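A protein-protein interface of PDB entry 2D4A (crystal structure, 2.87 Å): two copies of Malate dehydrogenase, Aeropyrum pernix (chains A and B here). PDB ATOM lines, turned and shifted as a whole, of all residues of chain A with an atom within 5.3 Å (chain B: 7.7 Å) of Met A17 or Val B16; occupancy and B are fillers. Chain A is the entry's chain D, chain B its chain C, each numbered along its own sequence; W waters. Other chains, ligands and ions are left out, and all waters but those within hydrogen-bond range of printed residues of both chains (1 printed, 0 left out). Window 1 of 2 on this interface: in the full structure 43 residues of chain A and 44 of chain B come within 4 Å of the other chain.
Val A16 touches Met B17, and with the chains exchanged Met A17 touches Val B16. Met A17 touches Met B20, and with the chains exchanged Met A20 touches Met B17. Met A20 touches its own counterpart, Met B20. Met A20 touches Arg B21, but with the chains exchanged Arg A21 does not touch Met B20 (4.2 Å).
The side-chain hydroxyl (OH) of Tyr A223 sits close to the side-chain sulfur (SD) of Met B12, 3.5 Å away. OD2 of Asp B42 is in hydrogen-bond range of N of Tyr A223 (2.8 Å).
Printed residues of chain A that touch a printed residue of chain B: Val A16, Met A17, Met A20, Arg A21, Tyr A223 and Ala A227. Among the printed residues, 14 pairs touch across the chains. Among the printed residues, no Asp or Glu carboxylate lies within 4 Å of a Lys or Arg side-chain nitrogen of the other chain.
Water W1 bridges the guanidinium group of Arg A21 (2.7 Å) and the backbone carbonyl oxygen of Met B20 (3.1 Å).
Among the printed residues, pairs that only touch across the chains: Val A16 with Met B17 (3.9 Å), Met A17 with Val B16 (3.6 Å), Met A17 with Met B20 (3.4 Å), Met A20 with Met B17 (3.8 Å), Met A20 with Met B20 (3.2 Å), Met A20 with Arg B21 (3.97 Å), Arg A21 with Leu B50 (3.6 Å), Tyr A223 with Val B16 (3.8 Å), Tyr A223 with Leu B43 (3.6 Å), Tyr A223 with Ala B46 (3.9 Å), Ala A227 with Ala B46 (3.7 Å) and Ala A227 with Glu B49 (3.3 Å).
Of chain A, only Met A17 and Tyr A223 come within 4 Å of Val B16. Of the printed residues of chain A, Met B12 touches Tyr A223 (3.1 Å). Printed residues of chain B within 4 Å of Met A20: Met B17, Met B20 and Arg B21. Of the printed residues of chain A, Leu B50 touches Arg A21. Of the printed residues of chain A, Leu B43 touches Tyr A223. Met A19 touches none of the printed residues of chain B. Leu A18 touches none of the printed residues of chain B. The nearest printed residue of chain B that does not touch Met A17 is Met B19 (4.7 Å). The nearest printed residue of chain A that does not touch Glu B49 is Tyr A223 (4.3 Å).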
ATOM      1  N   MET A  12      -3.365  22.835  -7.751  1.00  0.00           N
ATOM      2  CA  MET A  12      -2.418  23.685  -7.044  1.00  0.00           C
ATOM      3  C   MET A  12      -2.794  23.896  -5.592  1.00  0.00           C
ATOM      4  O   MET A  12      -1.923  24.090  -4.740  1.00  0.00           O
ATOM      5  CB  MET A  12      -2.261  25.032  -7.753  1.00  0.00           C
ATOM      6  CG  MET A  12      -1.316  24.970  -8.941  1.00  0.00           C
ATOM      7  SD  MET A  12       0.264  24.176  -8.446  1.00  0.00           S
ATOM      8  CE  MET A  12       0.290  22.849  -9.600  1.00  0.00           C
ATOM      9  N   ALA A  13      -4.084  23.864  -5.293  1.00  0.00           N
ATOM     10  CA  ALA A  13      -4.494  24.034  -3.905  1.00  0.00           C
ATOM     11  C   ALA A  13      -4.064  22.764  -3.150  1.00  0.00           C
ATOM     12  O   ALA A  13      -3.589  22.844  -2.022  1.00  0.00           O
ATOM     13  CB  ALA A  13      -6.008  24.235  -3.821  1.00  0.00           C
ATOM     14  N   THR A  14      -4.223  21.607  -3.805  1.00  0.00           N
ATOM     15  CA  THR A  14      -3.860  20.293  -3.259  1.00  0.00           C
ATOM     16  C   THR A  14      -2.353  20.233  -2.996  1.00  0.00           C
ATOM     17  O   THR A  14      -1.904  19.729  -1.964  1.00  0.00           O
ATOM     18  CB  THR A  14      -4.213  19.150  -4.255  1.00  0.00           C
ATOM     19  OG1 THR A  14      -5.546  19.336  -4.734  1.00  0.00           O
ATOM     20  CG2 THR A  14      -4.108  17.774  -3.589  1.00  0.00           C
ATOM     21  N   ALA A  15      -1.575  20.734  -3.947  1.00  0.00           N
ATOM     22  CA  ALA A  15      -0.131  20.735  -3.798  1.00  0.00           C
ATOM     23  C   ALA A  15       0.260  21.594  -2.596  1.00  0.00           C
ATOM     24  O   ALA A  15       1.075  21.178  -1.778  1.00  0.00           O
ATOM     25  CB  ALA A  15       0.539  21.260  -5.072  1.00  0.00           C
ATOM     26  N   VAL A  16      -0.331  22.784  -2.482  1.00  0.00           N
ATOM     27  CA  VAL A  16      -0.016  23.673  -1.364  1.00  0.00           C
ATOM     28  C   VAL A  16      -0.269  22.990  -0.021  1.00  0.00           C
ATOM     29  O   VAL A  16       0.601  22.976   0.859  1.00  0.00           O
ATOM     30  CB  VAL A  16      -0.847  24.991  -1.402  1.00  0.00           C
ATOM     31  CG1 VAL A  16      -0.581  25.820  -0.145  1.00  0.00           C
ATOM     32  CG2 VAL A  16      -0.488  25.802  -2.626  1.00  0.00           C
ATOM     33  N   MET A  17      -1.457  22.420   0.136  1.00  0.00           N
ATOM     34  CA  MET A  17      -1.814  21.754   1.379  1.00  0.00           C
ATOM     35  C   MET A  17      -0.956  20.515   1.658  1.00  0.00           C
ATOM     36  O   MET A  17      -0.633  20.232   2.812  1.00  0.00           O
ATOM     37  CB  MET A  17      -3.315  21.425   1.371  1.00  0.00           C
ATOM     38  CG  MET A  17      -4.196  22.677   1.375  1.00  0.00           C
ATOM     39  SD  MET A  17      -5.966  22.304   1.405  1.00  0.00           S
ATOM     40  CE  MET A  17      -6.647  23.742   0.595  1.00  0.00           C
ATOM     41  N   LEU A  18      -0.568  19.799   0.603  1.00  0.00           N
ATOM     42  CA  LEU A  18       0.279  18.608   0.739  1.00  0.00           C
ATOM     43  C   LEU A  18       1.697  18.989   1.149  1.00  0.00           C
ATOM     44  O   LEU A  18       2.347  18.267   1.895  1.00  0.00           O
ATOM     45  CB  LEU A  18       0.320  17.819  -0.575  1.00  0.00           C
ATOM     46  CG  LEU A  18      -0.834  16.833  -0.766  1.00  0.00           C
ATOM     47  CD1 LEU A  18      -0.797  16.201  -2.143  1.00  0.00           C
ATOM     48  CD2 LEU A  18      -0.748  15.787   0.328  1.00  0.00           C
ATOM     49  N   MET A  19       2.176  20.120   0.647  1.00  0.00           N
ATOM     50  CA  MET A  19       3.506  20.595   0.997  1.00  0.00           C
ATOM     51  C   MET A  19       3.512  20.943   2.497  1.00  0.00           C
ATOM     52  O   MET A  19       4.491  20.694   3.197  1.00  0.00           O
ATOM     53  CB  MET A  19       3.857  21.816   0.130  1.00  0.00           C
ATOM     54  CG  MET A  19       5.141  22.561   0.508  1.00  0.00           C
ATOM     55  SD  MET A  19       4.958  23.659   1.943  1.00  0.00           S
ATOM     56  CE  MET A  19       4.184  25.071   1.164  1.00  0.00           C
ATOM     57  N   MET A  20       2.409  21.505   2.984  1.00  0.00           N
ATOM     58  CA  MET A  20       2.277  21.861   4.394  1.00  0.00           C
ATOM     59  C   MET A  20       2.507  20.623   5.257  1.00  0.00           C
ATOM     60  O   MET A  20       3.376  20.620   6.114  1.00  0.00           O
ATOM     61  CB  MET A  20       0.870  22.404   4.679  1.00  0.00           C
ATOM     62  CG  MET A  20       0.484  23.714   3.988  1.00  0.00           C
ATOM     63  SD  MET A  20       1.334  25.143   4.658  1.00  0.00           S
ATOM     64  CE  MET A  20       0.856  25.072   6.392  1.00  0.00           C
ATOM     65  N   ARG A  21       1.726  19.575   5.014  1.00  0.00           N
ATOM     66  CA  ARG A  21       1.820  18.325   5.767  1.00  0.00           C
ATOM     67  C   ARG A  21       3.090  17.487   5.532  1.00  0.00           C
ATOM     68  O   ARG A  21       3.337  16.540   6.270  1.00  0.00           O
ATOM     69  CB  ARG A  21       0.601  17.456   5.457  1.00  0.00           C
ATOM     70  CG  ARG A  21      -0.729  18.028   5.922  1.00  0.00           C
ATOM     71  CD  ARG A  21      -0.924  17.789   7.405  1.00  0.00           C
ATOM     72  NE  ARG A  21      -2.090  18.478   7.961  1.00  0.00           N
ATOM     73  CZ  ARG A  21      -3.347  18.064   7.839  1.00  0.00           C
ATOM     74  NH1 ARG A  21      -3.623  16.949   7.171  1.00  0.00           N
ATOM     75  NH2 ARG A  21      -4.324  18.764   8.400  1.00  0.00           N
ATOM     76  N   TYR A 223     -10.847  24.463  -2.943  1.00  0.00           N
ATOM     77  CA  TYR A 223     -10.201  24.177  -1.664  1.00  0.00           C
ATOM     78  C   TYR A 223     -10.822  22.916  -1.044  1.00  0.00           C
ATOM     79  O   TYR A 223     -10.100  22.032  -0.580  1.00  0.00           O
ATOM     80  CB  TYR A 223     -10.309  25.357  -0.679  1.00  0.00           C
ATOM     81  CG  TYR A 223      -9.835  26.698  -1.217  1.00  0.00           C
ATOM     82  CD1 TYR A 223      -8.640  26.813  -1.935  1.00  0.00           C
ATOM     83  CD2 TYR A 223     -10.599  27.852  -1.024  1.00  0.00           C
ATOM     84  CE1 TYR A 223      -8.226  28.045  -2.454  1.00  0.00           C
ATOM     85  CE2 TYR A 223     -10.197  29.081  -1.536  1.00  0.00           C
ATOM     86  CZ  TYR A 223      -9.015  29.174  -2.253  1.00  0.00           C
ATOM     87  OH  TYR A 223      -8.646  30.388  -2.792  1.00  0.00           O
ATOM     88  N   ALA A 226      -9.461  19.752  -2.564  1.00  0.00           N
ATOM     89  CA  ALA A 226      -8.066  19.701  -2.118  1.00  0.00           C
ATOM     90  C   ALA A 226      -7.906  19.171  -0.688  1.00  0.00           C
ATOM     91  O   ALA A 226      -7.139  18.233  -0.452  1.00  0.00           O
ATOM     92  CB  ALA A 226      -7.439  21.083  -2.239  1.00  0.00           C
ATOM     93  N   ALA A 227      -8.622  19.771   0.259  1.00  0.00           N
ATOM     94  CA  ALA A 227      -8.562  19.333   1.644  1.00  0.00           C
ATOM     95  C   ALA A 227      -9.034  17.885   1.718  1.00  0.00           C
ATOM     96  O   ALA A 227      -8.596  17.107   2.568  1.00  0.00           O
ATOM     97  CB  ALA A 227      -9.439  20.210   2.510  1.00  0.00           C
ATOM     98  N   VAL A 230      -6.156  15.606   0.923  1.00  0.00           N
ATOM     99  CA  VAL A 230      -5.182  15.542   2.015  1.00  0.00           C
ATOM    100  C   VAL A 230      -5.525  14.366   2.951  1.00  0.00           C
ATOM    101  O   VAL A 230      -4.656  13.564   3.313  1.00  0.00           O
ATOM    102  CB  VAL A 230      -5.156  16.887   2.815  1.00  0.00           C
ATOM    103  CG1 VAL A 230      -4.227  16.794   4.024  1.00  0.00           C
ATOM    104  CG2 VAL A 230      -4.701  18.005   1.907  1.00  0.00           C
ATOM    105  N   ILE B   4      -7.061  39.784   6.116  1.00  0.00           N
ATOM    106  CA  ILE B   4      -6.347  39.708   4.849  1.00  0.00           C
ATOM    107  C   ILE B   4      -7.066  40.616   3.855  1.00  0.00           C
ATOM    108  O   ILE B   4      -8.272  40.501   3.647  1.00  0.00           O
ATOM    109  CB  ILE B   4      -6.324  38.259   4.303  1.00  0.00           C
ATOM    110  CG1 ILE B   4      -5.679  37.333   5.325  1.00  0.00           C
ATOM    111  CG2 ILE B   4      -5.523  38.179   3.025  1.00  0.00           C
ATOM    112  CD1 ILE B   4      -5.769  35.881   4.938  1.00  0.00           C
ATOM    113  N   LYS B   9      -4.542  35.962  -5.788  1.00  0.00           N
ATOM    114  CA  LYS B   9      -3.630  34.835  -5.662  1.00  0.00           C
ATOM    115  C   LYS B   9      -2.761  34.751  -4.412  1.00  0.00           C
ATOM    116  O   LYS B   9      -2.836  33.751  -3.698  1.00  0.00           O
ATOM    117  CB  LYS B   9      -2.785  34.719  -6.923  1.00  0.00           C
ATOM    118  CG  LYS B   9      -3.432  33.806  -7.931  1.00  0.00           C
ATOM    119  CD  LYS B   9      -3.087  34.175  -9.349  1.00  0.00           C
ATOM    120  CE  LYS B   9      -3.583  33.093 -10.299  1.00  0.00           C
ATOM    121  NZ  LYS B   9      -5.012  32.794 -10.017  1.00  0.00           N
ATOM    122  N   VAL B  10      -2.110  35.752  -4.262  1.00  0.00           N
ATOM    123  CA  VAL B  10      -1.261  35.710  -3.086  1.00  0.00           C
ATOM    124  C   VAL B  10      -2.085  35.779  -1.770  1.00  0.00           C
ATOM    125  O   VAL B  10      -1.702  35.194  -0.754  1.00  0.00           O
ATOM    126  CB  VAL B  10      -0.241  36.859  -3.134  1.00  0.00           C
ATOM    127  CG1 VAL B  10      -0.948  38.133  -3.428  1.00  0.00           C
ATOM    128  CG2 VAL B  10       0.440  37.021  -1.815  1.00  0.00           C
ATOM    129  N   GLY B  11      -3.204  36.347  -1.794  1.00  0.00           N
ATOM    130  CA  GLY B  11      -4.109  36.483  -0.667  1.00  0.00           C
ATOM    131  C   GLY B  11      -4.776  35.174  -0.284  1.00  0.00           C
ATOM    132  O   GLY B  11      -4.977  34.885   0.901  1.00  0.00           O
ATOM    133  N   MET B  12      -5.133  34.381  -1.289  1.00  0.00           N
ATOM    134  CA  MET B  12      -5.761  33.090  -1.049  1.00  0.00           C
ATOM    135  C   MET B  12      -4.744  32.035  -0.622  1.00  0.00           C
ATOM    136  O   MET B  12      -5.047  31.143   0.178  1.00  0.00           O
ATOM    137  CB  MET B  12      -6.512  32.631  -2.294  1.00  0.00           C
ATOM    138  CG  MET B  12      -7.788  33.403  -2.524  1.00  0.00           C
ATOM    139  SD  MET B  12      -8.816  33.397  -1.031  1.00  0.00           S
ATOM    140  CE  MET B  12      -8.961  35.078  -0.807  1.00  0.00           C
ATOM    141  N   ALA B  13      -3.532  32.139  -1.157  1.00  0.00           N
ATOM    142  CA  ALA B  13      -2.466  31.209  -0.804  1.00  0.00           C
ATOM    143  C   ALA B  13      -2.196  31.373   0.684  1.00  0.00           C
ATOM    144  O   ALA B  13      -1.977  30.396   1.397  1.00  0.00           O
ATOM    145  CB  ALA B  13      -1.212  31.534  -1.594  1.00  0.00           C
ATOM    146  N   THR B  14      -2.219  32.627   1.135  1.00  0.00           N
ATOM    147  CA  THR B  14      -1.976  32.978   2.532  1.00  0.00           C
ATOM    148  C   THR B  14      -3.115  32.463   3.380  1.00  0.00           C
ATOM    149  O   THR B  14      -2.899  31.926   4.464  1.00  0.00           O
ATOM    150  CB  THR B  14      -1.890  34.518   2.730  1.00  0.00           C
ATOM    151  OG1 THR B  14      -0.829  35.058   1.929  1.00  0.00           O
ATOM    152  CG2 THR B  14      -1.634  34.859   4.196  1.00  0.00           C
ATOM    153  N   ALA B  15      -4.335  32.639   2.888  1.00  0.00           N
ATOM    154  CA  ALA B  15      -5.517  32.183   3.615  1.00  0.00           C
ATOM    155  C   ALA B  15      -5.475  30.666   3.778  1.00  0.00           C
ATOM    156  O   ALA B  15      -5.746  30.145   4.856  1.00  0.00           O
ATOM    157  CB  ALA B  15      -6.777  32.601   2.871  1.00  0.00           C
ATOM    158  N   VAL B  16      -5.132  29.965   2.703  1.00  0.00           N
ATOM    159  CA  VAL B  16      -5.055  28.518   2.761  1.00  0.00           C
ATOM    160  C   VAL B  16      -4.024  28.060   3.772  1.00  0.00           C
ATOM    161  O   VAL B  16      -4.296  27.199   4.608  1.00  0.00           O
ATOM    162  CB  VAL B  16      -4.674  27.915   1.409  1.00  0.00           C
ATOM    163  CG1 VAL B  16      -4.432  26.415   1.556  1.00  0.00           C
ATOM    164  CG2 VAL B  16      -5.770  28.194   0.400  1.00  0.00           C
ATOM    165  N   MET B  17      -2.836  28.639   3.701  1.00  0.00           N
ATOM    166  CA  MET B  17      -1.773  28.250   4.611  1.00  0.00           C
ATOM    167  C   MET B  17      -2.057  28.587   6.071  1.00  0.00           C
ATOM    168  O   MET B  17      -1.683  27.820   6.960  1.00  0.00           O
ATOM    169  CB  MET B  17      -0.450  28.869   4.160  1.00  0.00           C
ATOM    170  CG  MET B  17       0.074  28.287   2.850  1.00  0.00           C
ATOM    171  SD  MET B  17       1.707  28.907   2.451  1.00  0.00           S
ATOM    172  CE  MET B  17       1.648  28.916   0.672  1.00  0.00           C
ATOM    173  N   LEU B  18      -2.723  29.716   6.320  1.00  0.00           N
ATOM    174  CA  LEU B  18      -3.056  30.137   7.688  1.00  0.00           C
ATOM    175  C   LEU B  18      -4.197  29.325   8.290  1.00  0.00           C
ATOM    176  O   LEU B  18      -4.307  29.209   9.512  1.00  0.00           O
ATOM    177  CB  LEU B  18      -3.415  31.629   7.734  1.00  0.00           C
ATOM    178  CG  LEU B  18      -2.262  32.633   7.837  1.00  0.00           C
ATOM    179  CD1 LEU B  18      -2.785  34.053   7.658  1.00  0.00           C
ATOM    180  CD2 LEU B  18      -1.584  32.468   9.190  1.00  0.00           C
ATOM    181  N   MET B  19      -5.054  28.774   7.437  1.00  0.00           N
ATOM    182  CA  MET B  19      -6.154  27.959   7.926  1.00  0.00           C
ATOM    183  C   MET B  19      -5.565  26.634   8.407  1.00  0.00           C
ATOM    184  O   MET B  19      -5.994  26.097   9.423  1.00  0.00           O
ATOM    185  CB  MET B  19      -7.184  27.744   6.811  1.00  0.00           C
ATOM    186  CG  MET B  19      -8.295  26.749   7.127  1.00  0.00           C
ATOM    187  SD  MET B  19      -7.838  25.031   6.783  1.00  0.00           S
ATOM    188  CE  MET B  19      -7.652  25.056   4.982  1.00  0.00           C
ATOM    189  N   MET B  20      -4.568  26.135   7.674  1.00  0.00           N
ATOM    190  CA  MET B  20      -3.866  24.887   7.983  1.00  0.00           C
ATOM    191  C   MET B  20      -3.239  24.911   9.369  1.00  0.00           C
ATOM    192  O   MET B  20      -3.266  23.919  10.090  1.00  0.00           O
ATOM    193  CB  MET B  20      -2.727  24.656   6.992  1.00  0.00           C
ATOM    194  CG  MET B  20      -3.115  24.475   5.545  1.00  0.00           C
ATOM    195  SD  MET B  20      -3.765  22.859   5.238  1.00  0.00           S
ATOM    196  CE  MET B  20      -2.262  21.881   5.302  1.00  0.00           C
ATOM    197  N   ARG B  21      -2.629  26.043   9.708  1.00  0.00           N
ATOM    198  CA  ARG B  21      -1.959  26.220  10.995  1.00  0.00           C
ATOM    199  C   ARG B  21      -2.948  26.490  12.126  1.00  0.00           C
ATOM    200  O   ARG B  21      -2.751  26.031  13.249  1.00  0.00           O
ATOM    201  CB  ARG B  21      -0.949  27.370  10.901  1.00  0.00           C
ATOM    202  CG  ARG B  21       0.290  27.070  10.059  1.00  0.00           C
ATOM    203  CD  ARG B  21       1.320  26.315  10.874  1.00  0.00           C
ATOM    204  NE  ARG B  21       2.297  25.608  10.053  1.00  0.00           N
ATOM    205  CZ  ARG B  21       3.531  26.033   9.814  1.00  0.00           C
ATOM    206  NH1 ARG B  21       3.954  27.176  10.336  1.00  0.00           N
ATOM    207  NH2 ARG B  21       4.342  25.308   9.055  1.00  0.00           N
ATOM    208  N   GLY B  22      -4.000  27.247  11.837  1.00  0.00           N
ATOM    209  CA  GLY B  22      -4.995  27.530  12.853  1.00  0.00           C
ATOM    210  C   GLY B  22      -4.534  28.434  13.979  1.00  0.00           C
ATOM    211  O   GLY B  22      -4.868  28.205  15.141  1.00  0.00           O
ATOM    212  N   LEU B  26      -9.576  34.105  10.688  1.00  0.00           N
ATOM    213  CA  LEU B  26      -9.138  35.027   9.656  1.00  0.00           C
ATOM    214  C   LEU B  26     -10.298  35.635   8.893  1.00  0.00           C
ATOM    215  O   LEU B  26     -11.336  35.006   8.717  1.00  0.00           O
ATOM    216  CB  LEU B  26      -8.126  34.361   8.716  1.00  0.00           C
ATOM    217  CG  LEU B  26      -8.398  33.122   7.872  1.00  0.00           C
ATOM    218  CD1 LEU B  26      -7.086  32.744   7.208  1.00  0.00           C
ATOM    219  CD2 LEU B  26      -8.906  31.961   8.707  1.00  0.00           C
ATOM    220  N   LEU B  28     -11.441  37.726   5.379  1.00  0.00           N
ATOM    221  CA  LEU B  28     -11.112  38.045   3.999  1.00  0.00           C
ATOM    222  C   LEU B  28     -11.892  39.284   3.611  1.00  0.00           C
ATOM    223  O   LEU B  28     -13.107  39.341   3.789  1.00  0.00           O
ATOM    224  CB  LEU B  28     -11.504  36.898   3.068  1.00  0.00           C
ATOM    225  CG  LEU B  28     -10.438  35.841   2.799  1.00  0.00           C
ATOM    226  CD1 LEU B  28      -9.267  36.492   2.066  1.00  0.00           C
ATOM    227  CD2 LEU B  28      -9.984  35.227   4.099  1.00  0.00           C
ATOM    228  N   ASP B  42     -15.698  28.368   0.449  1.00  0.00           N
ATOM    229  CA  ASP B  42     -14.969  27.203  -0.032  1.00  0.00           C
ATOM    230  C   ASP B  42     -13.838  26.911   0.951  1.00  0.00           C
ATOM    231  O   ASP B  42     -13.567  25.754   1.261  1.00  0.00           O
ATOM    232  CB  ASP B  42     -14.414  27.478  -1.437  1.00  0.00           C
ATOM    233  CG  ASP B  42     -13.756  26.257  -2.063  1.00  0.00           C
ATOM    234  OD1 ASP B  42     -14.199  25.120  -1.788  1.00  0.00           O
ATOM    235  OD2 ASP B  42     -12.805  26.430  -2.852  1.00  0.00           O
ATOM    236  N   LEU B  43     -13.200  27.963   1.459  1.00  0.00           N
ATOM    237  CA  LEU B  43     -12.114  27.779   2.402  1.00  0.00           C
ATOM    238  C   LEU B  43     -12.632  27.241   3.729  1.00  0.00           C
ATOM    239  O   LEU B  43     -11.917  26.534   4.455  1.00  0.00           O
ATOM    240  CB  LEU B  43     -11.345  29.087   2.617  1.00  0.00           C
ATOM    241  CG  LEU B  43     -10.100  28.998   3.519  1.00  0.00           C
ATOM    242  CD1 LEU B  43      -9.157  27.909   3.022  1.00  0.00           C
ATOM    243  CD2 LEU B  43      -9.387  30.355   3.547  1.00  0.00           C
ATOM    244  N   ALA B  46     -13.132  23.479   3.491  1.00  0.00           N
ATOM    245  CA  ALA B  46     -11.848  22.788   3.591  1.00  0.00           C
ATOM    246  C   ALA B  46     -11.495  22.594   5.074  1.00  0.00           C
ATOM    247  O   ALA B  46     -11.188  21.483   5.498  1.00  0.00           O
ATOM    248  CB  ALA B  46     -10.762  23.598   2.885  1.00  0.00           C
ATOM    249  N   ALA B  47     -11.550  23.673   5.858  1.00  0.00           N
ATOM    250  CA  ALA B  47     -11.243  23.606   7.286  1.00  0.00           C
ATOM    251  C   ALA B  47     -12.109  22.576   8.001  1.00  0.00           C
ATOM    252  O   ALA B  47     -11.677  21.953   8.977  1.00  0.00           O
ATOM    253  CB  ALA B  47     -11.434  24.970   7.932  1.00  0.00           C
ATOM    254  N   GLU B  49     -13.150  19.744   6.772  1.00  0.00           N
ATOM    255  CA  GLU B  49     -12.659  18.407   6.442  1.00  0.00           C
ATOM    256  C   GLU B  49     -11.383  18.140   7.224  1.00  0.00           C
ATOM    257  O   GLU B  49     -11.124  17.017   7.658  1.00  0.00           O
ATOM    258  CB  GLU B  49     -12.332  18.304   4.959  1.00  0.00           C
ATOM    259  CG  GLU B  49     -13.448  18.744   4.059  1.00  0.00           C
ATOM    260  CD  GLU B  49     -13.044  18.722   2.605  1.00  0.00           C
ATOM    261  OE1 GLU B  49     -13.090  17.643   1.991  1.00  0.00           O
ATOM    262  OE2 GLU B  49     -12.664  19.787   2.083  1.00  0.00           O
ATOM    263  N   LEU B  50     -10.582  19.189   7.374  1.00  0.00           N
ATOM    264  CA  LEU B  50      -9.326  19.109   8.090  1.00  0.00           C
ATOM    265  C   LEU B  50      -9.558  19.195   9.590  1.00  0.00           C
ATOM    266  O   LEU B  50      -8.660  18.918  10.384  1.00  0.00           O
ATOM    267  CB  LEU B  50      -8.390  20.234   7.640  1.00  0.00           C
ATOM    268  CG  LEU B  50      -7.851  20.077   6.224  1.00  0.00           C
ATOM    269  CD1 LEU B  50      -6.914  21.216   5.896  1.00  0.00           C
ATOM    270  CD2 LEU B  50      -7.128  18.744   6.118  1.00  0.00           C
ATOM    271  N   ILE B  56     -13.749  31.449   9.832  1.00  0.00           N
ATOM    272  CA  ILE B  56     -13.289  31.962   8.544  1.00  0.00           C
ATOM    273  C   ILE B  56     -14.423  32.678   7.825  1.00  0.00           C
ATOM    274  O   ILE B  56     -15.459  32.075   7.577  1.00  0.00           O
ATOM    275  CB  ILE B  56     -12.820  30.827   7.609  1.00  0.00           C
ATOM    276  CG1 ILE B  56     -11.698  30.018   8.247  1.00  0.00           C
ATOM    277  CG2 ILE B  56     -12.340  31.409   6.296  1.00  0.00           C
ATOM    278  CD1 ILE B  56     -11.130  28.960   7.307  1.00  0.00           C
ATOM    279  N   ALA B 226       3.271  34.107   0.500  1.00  0.00           N
ATOM    280  CA  ALA B 226       2.257  33.512   1.367  1.00  0.00           C
ATOM    281  C   ALA B 226       2.911  32.796   2.541  1.00  0.00           C
ATOM    282  O   ALA B 226       2.607  33.079   3.706  1.00  0.00           O
ATOM    283  CB  ALA B 226       1.395  32.540   0.571  1.00  0.00           C
ATOM    284  N   VAL B 230       3.147  33.452   6.802  1.00  0.00           N
ATOM    285  CA  VAL B 230       2.842  32.517   7.863  1.00  0.00           C
ATOM    286  C   VAL B 230       3.908  32.661   8.945  1.00  0.00           C
ATOM    287  O   VAL B 230       3.589  32.781  10.125  1.00  0.00           O
ATOM    288  CB  VAL B 230       2.830  31.064   7.363  1.00  0.00           C
ATOM    289  CG1 VAL B 230       2.662  30.122   8.547  1.00  0.00           C
ATOM    290  CG2 VAL B 230       1.690  30.857   6.379  1.00  0.00           C
HETATM  291  O   HOH W   1      -2.938  20.913   9.257  1.00  0.00           O
